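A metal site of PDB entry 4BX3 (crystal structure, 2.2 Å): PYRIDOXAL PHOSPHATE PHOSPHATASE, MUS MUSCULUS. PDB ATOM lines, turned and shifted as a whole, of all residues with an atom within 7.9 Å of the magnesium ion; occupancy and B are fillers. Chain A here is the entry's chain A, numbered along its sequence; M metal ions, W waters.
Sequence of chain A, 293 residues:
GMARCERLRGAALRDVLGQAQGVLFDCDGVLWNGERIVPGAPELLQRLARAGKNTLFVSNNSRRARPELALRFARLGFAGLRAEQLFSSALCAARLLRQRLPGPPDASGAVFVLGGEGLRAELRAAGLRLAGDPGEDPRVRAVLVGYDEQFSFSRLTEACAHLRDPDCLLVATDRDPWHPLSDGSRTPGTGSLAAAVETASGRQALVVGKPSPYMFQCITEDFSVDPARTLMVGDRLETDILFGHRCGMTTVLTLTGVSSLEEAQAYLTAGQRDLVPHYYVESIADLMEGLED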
ATOM      1  N   ASP A  26       8.975 -29.176   6.279  1.00  0.00           N
ATOM      2  CA  ASP A  26       9.144 -28.179   5.215  1.00  0.00           C
ATOM      3  C   ASP A  26       8.085 -27.087   5.482  1.00  0.00           C
ATOM      4  O   ASP A  26       7.097 -27.349   6.217  1.00  0.00           O
ATOM      5  CB  ASP A  26       8.952 -28.849   3.840  1.00  0.00           C
ATOM      6  CG  ASP A  26       8.983 -27.871   2.674  1.00  0.00           C
ATOM      7  OD1 ASP A  26       9.821 -26.927   2.597  1.00  0.00           O
ATOM      8  OD2 ASP A  26       8.039 -28.011   1.879  1.00  0.00           O
ATOM      9  N   CYS A  27       8.268 -25.903   4.902  1.00  0.00           N
ATOM     10  CA  CYS A  27       7.385 -24.780   5.194  1.00  0.00           C
ATOM     11  C   CYS A  27       6.311 -24.523   4.128  1.00  0.00           C
ATOM     12  O   CYS A  27       5.135 -24.767   4.385  1.00  0.00           O
ATOM     13  CB  CYS A  27       8.230 -23.519   5.463  1.00  0.00           C
ATOM     14  SG  CYS A  27       9.276 -23.719   6.993  1.00  0.00           S
ATOM     15  N   ASP A  28       6.711 -24.063   2.949  1.00  0.00           N
ATOM     16  CA  ASP A  28       5.761 -23.728   1.889  1.00  0.00           C
ATOM     17  C   ASP A  28       5.018 -24.979   1.400  1.00  0.00           C
ATOM     18  O   ASP A  28       5.625 -25.997   1.119  1.00  0.00           O
ATOM     19  CB  ASP A  28       6.465 -23.051   0.692  1.00  0.00           C
ATOM     20  CG  ASP A  28       7.279 -21.797   1.094  1.00  0.00           C
ATOM     21  OD1 ASP A  28       6.998 -21.184   2.131  1.00  0.00           O
ATOM     22  OD2 ASP A  28       8.153 -21.360   0.337  1.00  0.00           O
ATOM     23  N   GLY A  29       3.701 -24.886   1.298  1.00  0.00           N
ATOM     24  CA  GLY A  29       2.886 -26.018   0.915  1.00  0.00           C
ATOM     25  C   GLY A  29       2.550 -26.963   2.074  1.00  0.00           C
ATOM     26  O   GLY A  29       1.739 -27.859   1.887  1.00  0.00           O
ATOM     27  N   VAL A  30       3.144 -26.742   3.255  1.00  0.00           N
ATOM     28  CA  VAL A  30       2.987 -27.655   4.397  1.00  0.00           C
ATOM     29  C   VAL A  30       2.360 -26.935   5.633  1.00  0.00           C
ATOM     30  O   VAL A  30       1.399 -27.412   6.217  1.00  0.00           O
ATOM     31  CB  VAL A  30       4.360 -28.279   4.805  1.00  0.00           C
ATOM     32  CG1 VAL A  30       4.218 -29.178   6.008  1.00  0.00           C
ATOM     33  CG2 VAL A  30       4.991 -29.050   3.609  1.00  0.00           C
ATOM     34  N   LEU A  31       2.951 -25.829   6.045  1.00  0.00           N
ATOM     35  CA  LEU A  31       2.406 -25.044   7.130  1.00  0.00           C
ATOM     36  C   LEU A  31       1.465 -23.960   6.596  1.00  0.00           C
ATOM     37  O   LEU A  31       0.573 -23.496   7.299  1.00  0.00           O
ATOM     38  CB  LEU A  31       3.528 -24.357   7.909  1.00  0.00           C
ATOM     39  CG  LEU A  31       4.616 -25.254   8.460  1.00  0.00           C
ATOM     40  CD1 LEU A  31       5.695 -24.384   9.066  1.00  0.00           C
ATOM     41  CD2 LEU A  31       4.048 -26.148   9.507  1.00  0.00           C
ATOM     42  N   TRP A  32       1.731 -23.538   5.365  1.00  0.00           N
ATOM     43  CA  TRP A  32       0.941 -22.499   4.710  1.00  0.00           C
ATOM     44  C   TRP A  32       1.038 -22.598   3.191  1.00  0.00           C
ATOM     45  O   TRP A  32       1.914 -23.261   2.663  1.00  0.00           O
ATOM     46  CB  TRP A  32       1.435 -21.111   5.126  1.00  0.00           C
ATOM     47  CG  TRP A  32       2.926 -20.903   4.926  1.00  0.00           C
ATOM     48  CD1 TRP A  32       3.601 -20.830   3.722  1.00  0.00           C
ATOM     49  CD2 TRP A  32       3.910 -20.695   5.939  1.00  0.00           C
ATOM     50  NE1 TRP A  32       4.942 -20.599   3.946  1.00  0.00           N
ATOM     51  CE2 TRP A  32       5.168 -20.538   5.293  1.00  0.00           C
ATOM     52  CE3 TRP A  32       3.869 -20.654   7.327  1.00  0.00           C
ATOM     53  CZ2 TRP A  32       6.366 -20.333   5.994  1.00  0.00           C
ATOM     54  CZ3 TRP A  32       5.070 -20.455   8.035  1.00  0.00           C
ATOM     55  CH2 TRP A  32       6.298 -20.288   7.356  1.00  0.00           C
ATOM     56  N   ASN A  33       0.136 -21.899   2.511  1.00  0.00           N
ATOM     57  CA  ASN A  33       0.222 -21.652   1.080  1.00  0.00           C
ATOM     58  C   ASN A  33       0.081 -20.158   0.859  1.00  0.00           C
ATOM     59  O   ASN A  33      -1.022 -19.623   1.068  1.00  0.00           O
ATOM     60  CB  ASN A  33      -0.902 -22.398   0.349  1.00  0.00           C
ATOM     61  CG  ASN A  33      -0.671 -23.912   0.260  1.00  0.00           C
ATOM     62  OD1 ASN A  33       0.221 -24.385  -0.463  1.00  0.00           O
ATOM     63  ND2 ASN A  33      -1.446 -24.668   1.008  1.00  0.00           N
ATOM     64  N   VAL A  58      12.703 -26.795   7.826  1.00  0.00           N
ATOM     65  CA  VAL A  58      13.703 -26.909   6.797  1.00  0.00           C
ATOM     66  C   VAL A  58      13.043 -26.477   5.473  1.00  0.00           C
ATOM     67  O   VAL A  58      12.009 -27.003   5.106  1.00  0.00           O
ATOM     68  CB  VAL A  58      14.207 -28.368   6.792  1.00  0.00           C
ATOM     69  CG1 VAL A  58      13.194 -29.216   6.033  1.00  0.00           C
ATOM     70  CG2 VAL A  58      15.561 -28.490   6.213  1.00  0.00           C
ATOM     71  N   SER A  59      13.574 -25.441   4.826  1.00  0.00           N
ATOM     72  CA  SER A  59      12.972 -24.837   3.674  1.00  0.00           C
ATOM     73  C   SER A  59      13.989 -24.536   2.596  1.00  0.00           C
ATOM     74  O   SER A  59      15.129 -24.160   2.926  1.00  0.00           O
ATOM     75  CB  SER A  59      12.345 -23.512   4.098  1.00  0.00           C
ATOM     76  OG  SER A  59      11.721 -22.931   2.964  1.00  0.00           O
ATOM     77  N   ASN A  60      13.592 -24.661   1.318  1.00  0.00           N
ATOM     78  CA  ASN A  60      14.501 -24.273   0.240  1.00  0.00           C
ATOM     79  C   ASN A  60      14.326 -22.821  -0.167  1.00  0.00           C
ATOM     80  O   ASN A  60      15.113 -22.281  -0.949  1.00  0.00           O
ATOM     81  CB  ASN A  60      14.384 -25.221  -0.987  1.00  0.00           C
ATOM     82  CG  ASN A  60      15.183 -26.498  -0.799  1.00  0.00           C
ATOM     83  OD1 ASN A  60      16.008 -26.621   0.109  1.00  0.00           O
ATOM     84  ND2 ASN A  60      14.912 -27.479  -1.632  1.00  0.00           N
ATOM     85  N   ASP A 176      15.192 -26.838  -6.812  1.00  0.00           N
ATOM     86  CA  ASP A 176      13.773 -26.866  -7.107  1.00  0.00           C
ATOM     87  C   ASP A 176      13.516 -26.188  -8.500  1.00  0.00           C
ATOM     88  O   ASP A 176      14.019 -25.129  -8.781  1.00  0.00           O
ATOM     89  CB  ASP A 176      12.995 -26.156  -6.030  1.00  0.00           C
ATOM     90  CG  ASP A 176      13.121 -26.839  -4.663  1.00  0.00           C
ATOM     91  OD1 ASP A 176      13.723 -27.937  -4.537  1.00  0.00           O
ATOM     92  OD2 ASP A 176      12.568 -26.289  -3.716  1.00  0.00           O
ATOM     93  N   HIS A 179       7.915 -23.147  -8.719  1.00  0.00           N
ATOM     94  CA  HIS A 179       7.047 -23.144  -7.526  1.00  0.00           C
ATOM     95  C   HIS A 179       5.679 -22.609  -7.914  1.00  0.00           C
ATOM     96  O   HIS A 179       5.593 -21.711  -8.703  1.00  0.00           O
ATOM     97  CB  HIS A 179       7.640 -22.265  -6.403  1.00  0.00           C
ATOM     98  CG  HIS A 179       9.045 -22.635  -6.062  1.00  0.00           C
ATOM     99  ND1 HIS A 179       9.351 -23.643  -5.177  1.00  0.00           N
ATOM    100  CD2 HIS A 179      10.230 -22.168  -6.552  1.00  0.00           C
ATOM    101  CE1 HIS A 179      10.667 -23.784  -5.129  1.00  0.00           C
ATOM    102  NE2 HIS A 179      11.220 -22.888  -5.917  1.00  0.00           N
ATOM    103  N   PRO A 180       4.615 -23.147  -7.305  1.00  0.00           N
ATOM    104  CA  PRO A 180       3.237 -22.679  -7.507  1.00  0.00           C
ATOM    105  C   PRO A 180       3.018 -21.310  -6.852  1.00  0.00           C
ATOM    106  O   PRO A 180       3.558 -21.036  -5.753  1.00  0.00           O
ATOM    107  CB  PRO A 180       2.407 -23.706  -6.739  1.00  0.00           C
ATOM    108  CG  PRO A 180       3.331 -24.007  -5.486  1.00  0.00           C
ATOM    109  CD  PRO A 180       4.743 -24.025  -6.130  1.00  0.00           C
ATOM    110  N   LYS A 210      17.664 -29.356   0.333  1.00  0.00           N
ATOM    111  CA  LYS A 210      17.046 -30.635   0.095  1.00  0.00           C
ATOM    112  C   LYS A 210      16.911 -30.832  -1.423  1.00  0.00           C
ATOM    113  O   LYS A 210      16.530 -29.893  -2.122  1.00  0.00           O
ATOM    114  CB  LYS A 210      15.630 -30.666   0.658  1.00  0.00           C
ATOM    115  CG  LYS A 210      15.497 -30.407   2.134  1.00  0.00           C
ATOM    116  CD  LYS A 210      14.022 -30.119   2.479  1.00  0.00           C
ATOM    117  CE  LYS A 210      13.492 -28.976   1.661  1.00  0.00           C
ATOM    118  NZ  LYS A 210      12.086 -28.640   1.944  1.00  0.00           N
ATOM    119  N   VAL A 233       8.485 -34.357   7.066  1.00  0.00           N
ATOM    120  CA  VAL A 233       7.143 -34.036   6.528  1.00  0.00           C
ATOM    121  C   VAL A 233       7.237 -32.933   5.451  1.00  0.00           C
ATOM    122  O   VAL A 233       7.734 -31.845   5.697  1.00  0.00           O
ATOM    123  CB  VAL A 233       6.213 -33.567   7.628  1.00  0.00           C
ATOM    124  CG1 VAL A 233       4.906 -33.195   7.088  1.00  0.00           C
ATOM    125  CG2 VAL A 233       6.075 -34.620   8.685  1.00  0.00           C
ATOM    126  N   GLY A 234       6.783 -33.244   4.252  1.00  0.00           N
ATOM    127  CA  GLY A 234       6.904 -32.352   3.109  1.00  0.00           C
ATOM    128  C   GLY A 234       5.795 -32.578   2.085  1.00  0.00           C
ATOM    129  O   GLY A 234       5.092 -33.570   2.142  1.00  0.00           O
ATOM    130  N   ASP A 235       5.651 -31.646   1.144  1.00  0.00           N
ATOM    131  CA  ASP A 235       4.648 -31.733   0.102  1.00  0.00           C
ATOM    132  C   ASP A 235       5.226 -32.119  -1.261  1.00  0.00           C
ATOM    133  O   ASP A 235       4.474 -32.288  -2.213  1.00  0.00           O
ATOM    134  CB  ASP A 235       3.930 -30.399  -0.050  1.00  0.00           C
ATOM    135  CG  ASP A 235       4.844 -29.270  -0.508  1.00  0.00           C
ATOM    136  OD1 ASP A 235       5.866 -29.012   0.168  1.00  0.00           O
ATOM    137  OD2 ASP A 235       4.517 -28.593  -1.521  1.00  0.00           O
ATOM    138  N   ARG A 236       6.548 -32.224  -1.366  1.00  0.00           N
ATOM    139  CA  ARG A 236       7.154 -32.439  -2.681  1.00  0.00           C
ATOM    140  C   ARG A 236       8.021 -33.705  -2.725  1.00  0.00           C
ATOM    141  O   ARG A 236       9.057 -33.807  -2.080  1.00  0.00           O
ATOM    142  CB  ARG A 236       7.988 -31.231  -3.036  1.00  0.00           C
ATOM    143  CG  ARG A 236       8.358 -31.109  -4.485  1.00  0.00           C
ATOM    144  CD  ARG A 236       8.752 -29.644  -4.748  1.00  0.00           C
ATOM    145  NE  ARG A 236       8.656 -29.368  -6.166  1.00  0.00           N
ATOM    146  CZ  ARG A 236       8.579 -28.170  -6.707  1.00  0.00           C
ATOM    147  NH1 ARG A 236       8.573 -27.073  -5.978  1.00  0.00           N
ATOM    148  NH2 ARG A 236       8.484 -28.080  -8.017  1.00  0.00           N
ATOM    149  N   THR A 239      11.838 -33.572  -3.606  1.00  0.00           N
ATOM    150  CA  THR A 239      12.710 -32.834  -2.707  1.00  0.00           C
ATOM    151  C   THR A 239      12.615 -33.335  -1.262  1.00  0.00           C
ATOM    152  O   THR A 239      13.596 -33.811  -0.710  1.00  0.00           O
ATOM    153  CB  THR A 239      12.472 -31.297  -2.748  1.00  0.00           C
ATOM    154  OG1 THR A 239      11.213 -30.979  -2.189  1.00  0.00           O
ATOM    155  CG2 THR A 239      12.533 -30.799  -4.138  1.00  0.00           C
ATOM    156  N   ASP A 240      11.417 -33.274  -0.669  1.00  0.00           N
ATOM    157  CA  ASP A 240      11.239 -33.603   0.736  1.00  0.00           C
ATOM    158  C   ASP A 240      11.392 -35.098   1.035  1.00  0.00           C
ATOM    159  O   ASP A 240      12.105 -35.506   1.979  1.00  0.00           O
ATOM    160  CB  ASP A 240       9.893 -33.041   1.194  1.00  0.00           C
ATOM    161  CG  ASP A 240       9.792 -31.518   0.952  1.00  0.00           C
ATOM    162  OD1 ASP A 240      10.819 -30.852   1.273  1.00  0.00           O
ATOM    163  OD2 ASP A 240       8.742 -30.992   0.432  1.00  0.00           O
ATOM    164  N   THR A 254       2.477 -34.768   2.837  1.00  0.00           N
ATOM    165  CA  THR A 254       1.199 -34.125   3.094  1.00  0.00           C
ATOM    166  C   THR A 254       0.608 -33.629   1.749  1.00  0.00           C
ATOM    167  O   THR A 254       1.349 -33.270   0.851  1.00  0.00           O
ATOM    168  CB  THR A 254       1.327 -32.982   4.104  1.00  0.00           C
ATOM    169  OG1 THR A 254       0.056 -32.334   4.210  1.00  0.00           O
ATOM    170  CG2 THR A 254       2.317 -31.928   3.671  1.00  0.00           C
ATOM    171  N   GLY A 257       0.096 -29.368  -0.822  1.00  0.00           N
ATOM    172  CA  GLY A 257       1.078 -28.663  -1.613  1.00  0.00           C
ATOM    173  C   GLY A 257       1.274 -29.199  -3.018  1.00  0.00           C
ATOM    174  O   GLY A 257       0.324 -29.542  -3.717  1.00  0.00           O
ATOM    175  N   VAL A 258       2.531 -29.263  -3.446  1.00  0.00           N
ATOM    176  CA  VAL A 258       2.863 -29.556  -4.836  1.00  0.00           C
ATOM    177  C   VAL A 258       2.503 -30.969  -5.282  1.00  0.00           C
ATOM    178  O   VAL A 258       1.846 -31.133  -6.303  1.00  0.00           O
ATOM    179  CB  VAL A 258       4.359 -29.302  -5.098  1.00  0.00           C
ATOM    180  CG1 VAL A 258       4.773 -29.836  -6.479  1.00  0.00           C
ATOM    181  CG2 VAL A 258       4.684 -27.831  -5.017  1.00  0.00           C
ATOM    182  N   SER A 259       2.942 -32.006  -4.583  1.00  0.00           N
ATOM    183  CA  SER A 259       2.747 -33.372  -5.109  1.00  0.00           C
ATOM    184  C   SER A 259       1.412 -33.971  -4.798  1.00  0.00           C
ATOM    185  O   SER A 259       0.764 -33.564  -3.842  1.00  0.00           O
ATOM    186  CB  SER A 259       3.744 -34.356  -4.519  1.00  0.00           C
ATOM    187  OG  SER A 259       5.062 -33.996  -4.760  1.00  0.00           O
HETATM  188 MG    MG M   1       7.053 -27.257   0.091  1.00  0.00          MG
HETATM  189  O   HOH W   1       6.277 -26.635  -1.727  1.00  0.00           O
HETATM  190  O   HOH W   2       8.519 -25.887   0.017  1.00  0.00           O
HETATM  191  O   HOH W   3       8.674 -28.626  -0.731  1.00  0.00           O
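Within 4 Å of the magnesium ion: Asp 26, Asp 28 and Asp 235.
The backbone NH (N) of Asp 235 is in hydrogen-bond range of the side-chain carboxylate (OD2) of Asp 240 (3.2 Å). The side-chain carboxylate of Asp 235 lies within hydrogen-bond range of the backbone NH of Val 258, 2.8 Å away. O of Asp 235 sits at hydrogen-bond distance from N of Ser 259 (2.8 Å). The side-chain carboxylate (OD1) of Asp 28 sits at hydrogen-bond distance from the indole nitrogen (NE1) of Trp 32 (2.8 Å). NZ of Lys 210 is in salt-bridge range of OD1 of Asp 26 (2.9 Å). The backbone NH (N) of Asp 26 sits at hydrogen-bond distance from the backbone carbonyl oxygen (O) of Val 233 (3.0 Å).
The magnesium ion is bound by water W2 (2.0 Å), water W1 (2.1 Å), OD1 of Asp 235 (2.1 Å), O of Asp 28 (2.2 Å), OD2 of Asp 26 (2.2 Å) and water W3 (2.3 Å).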
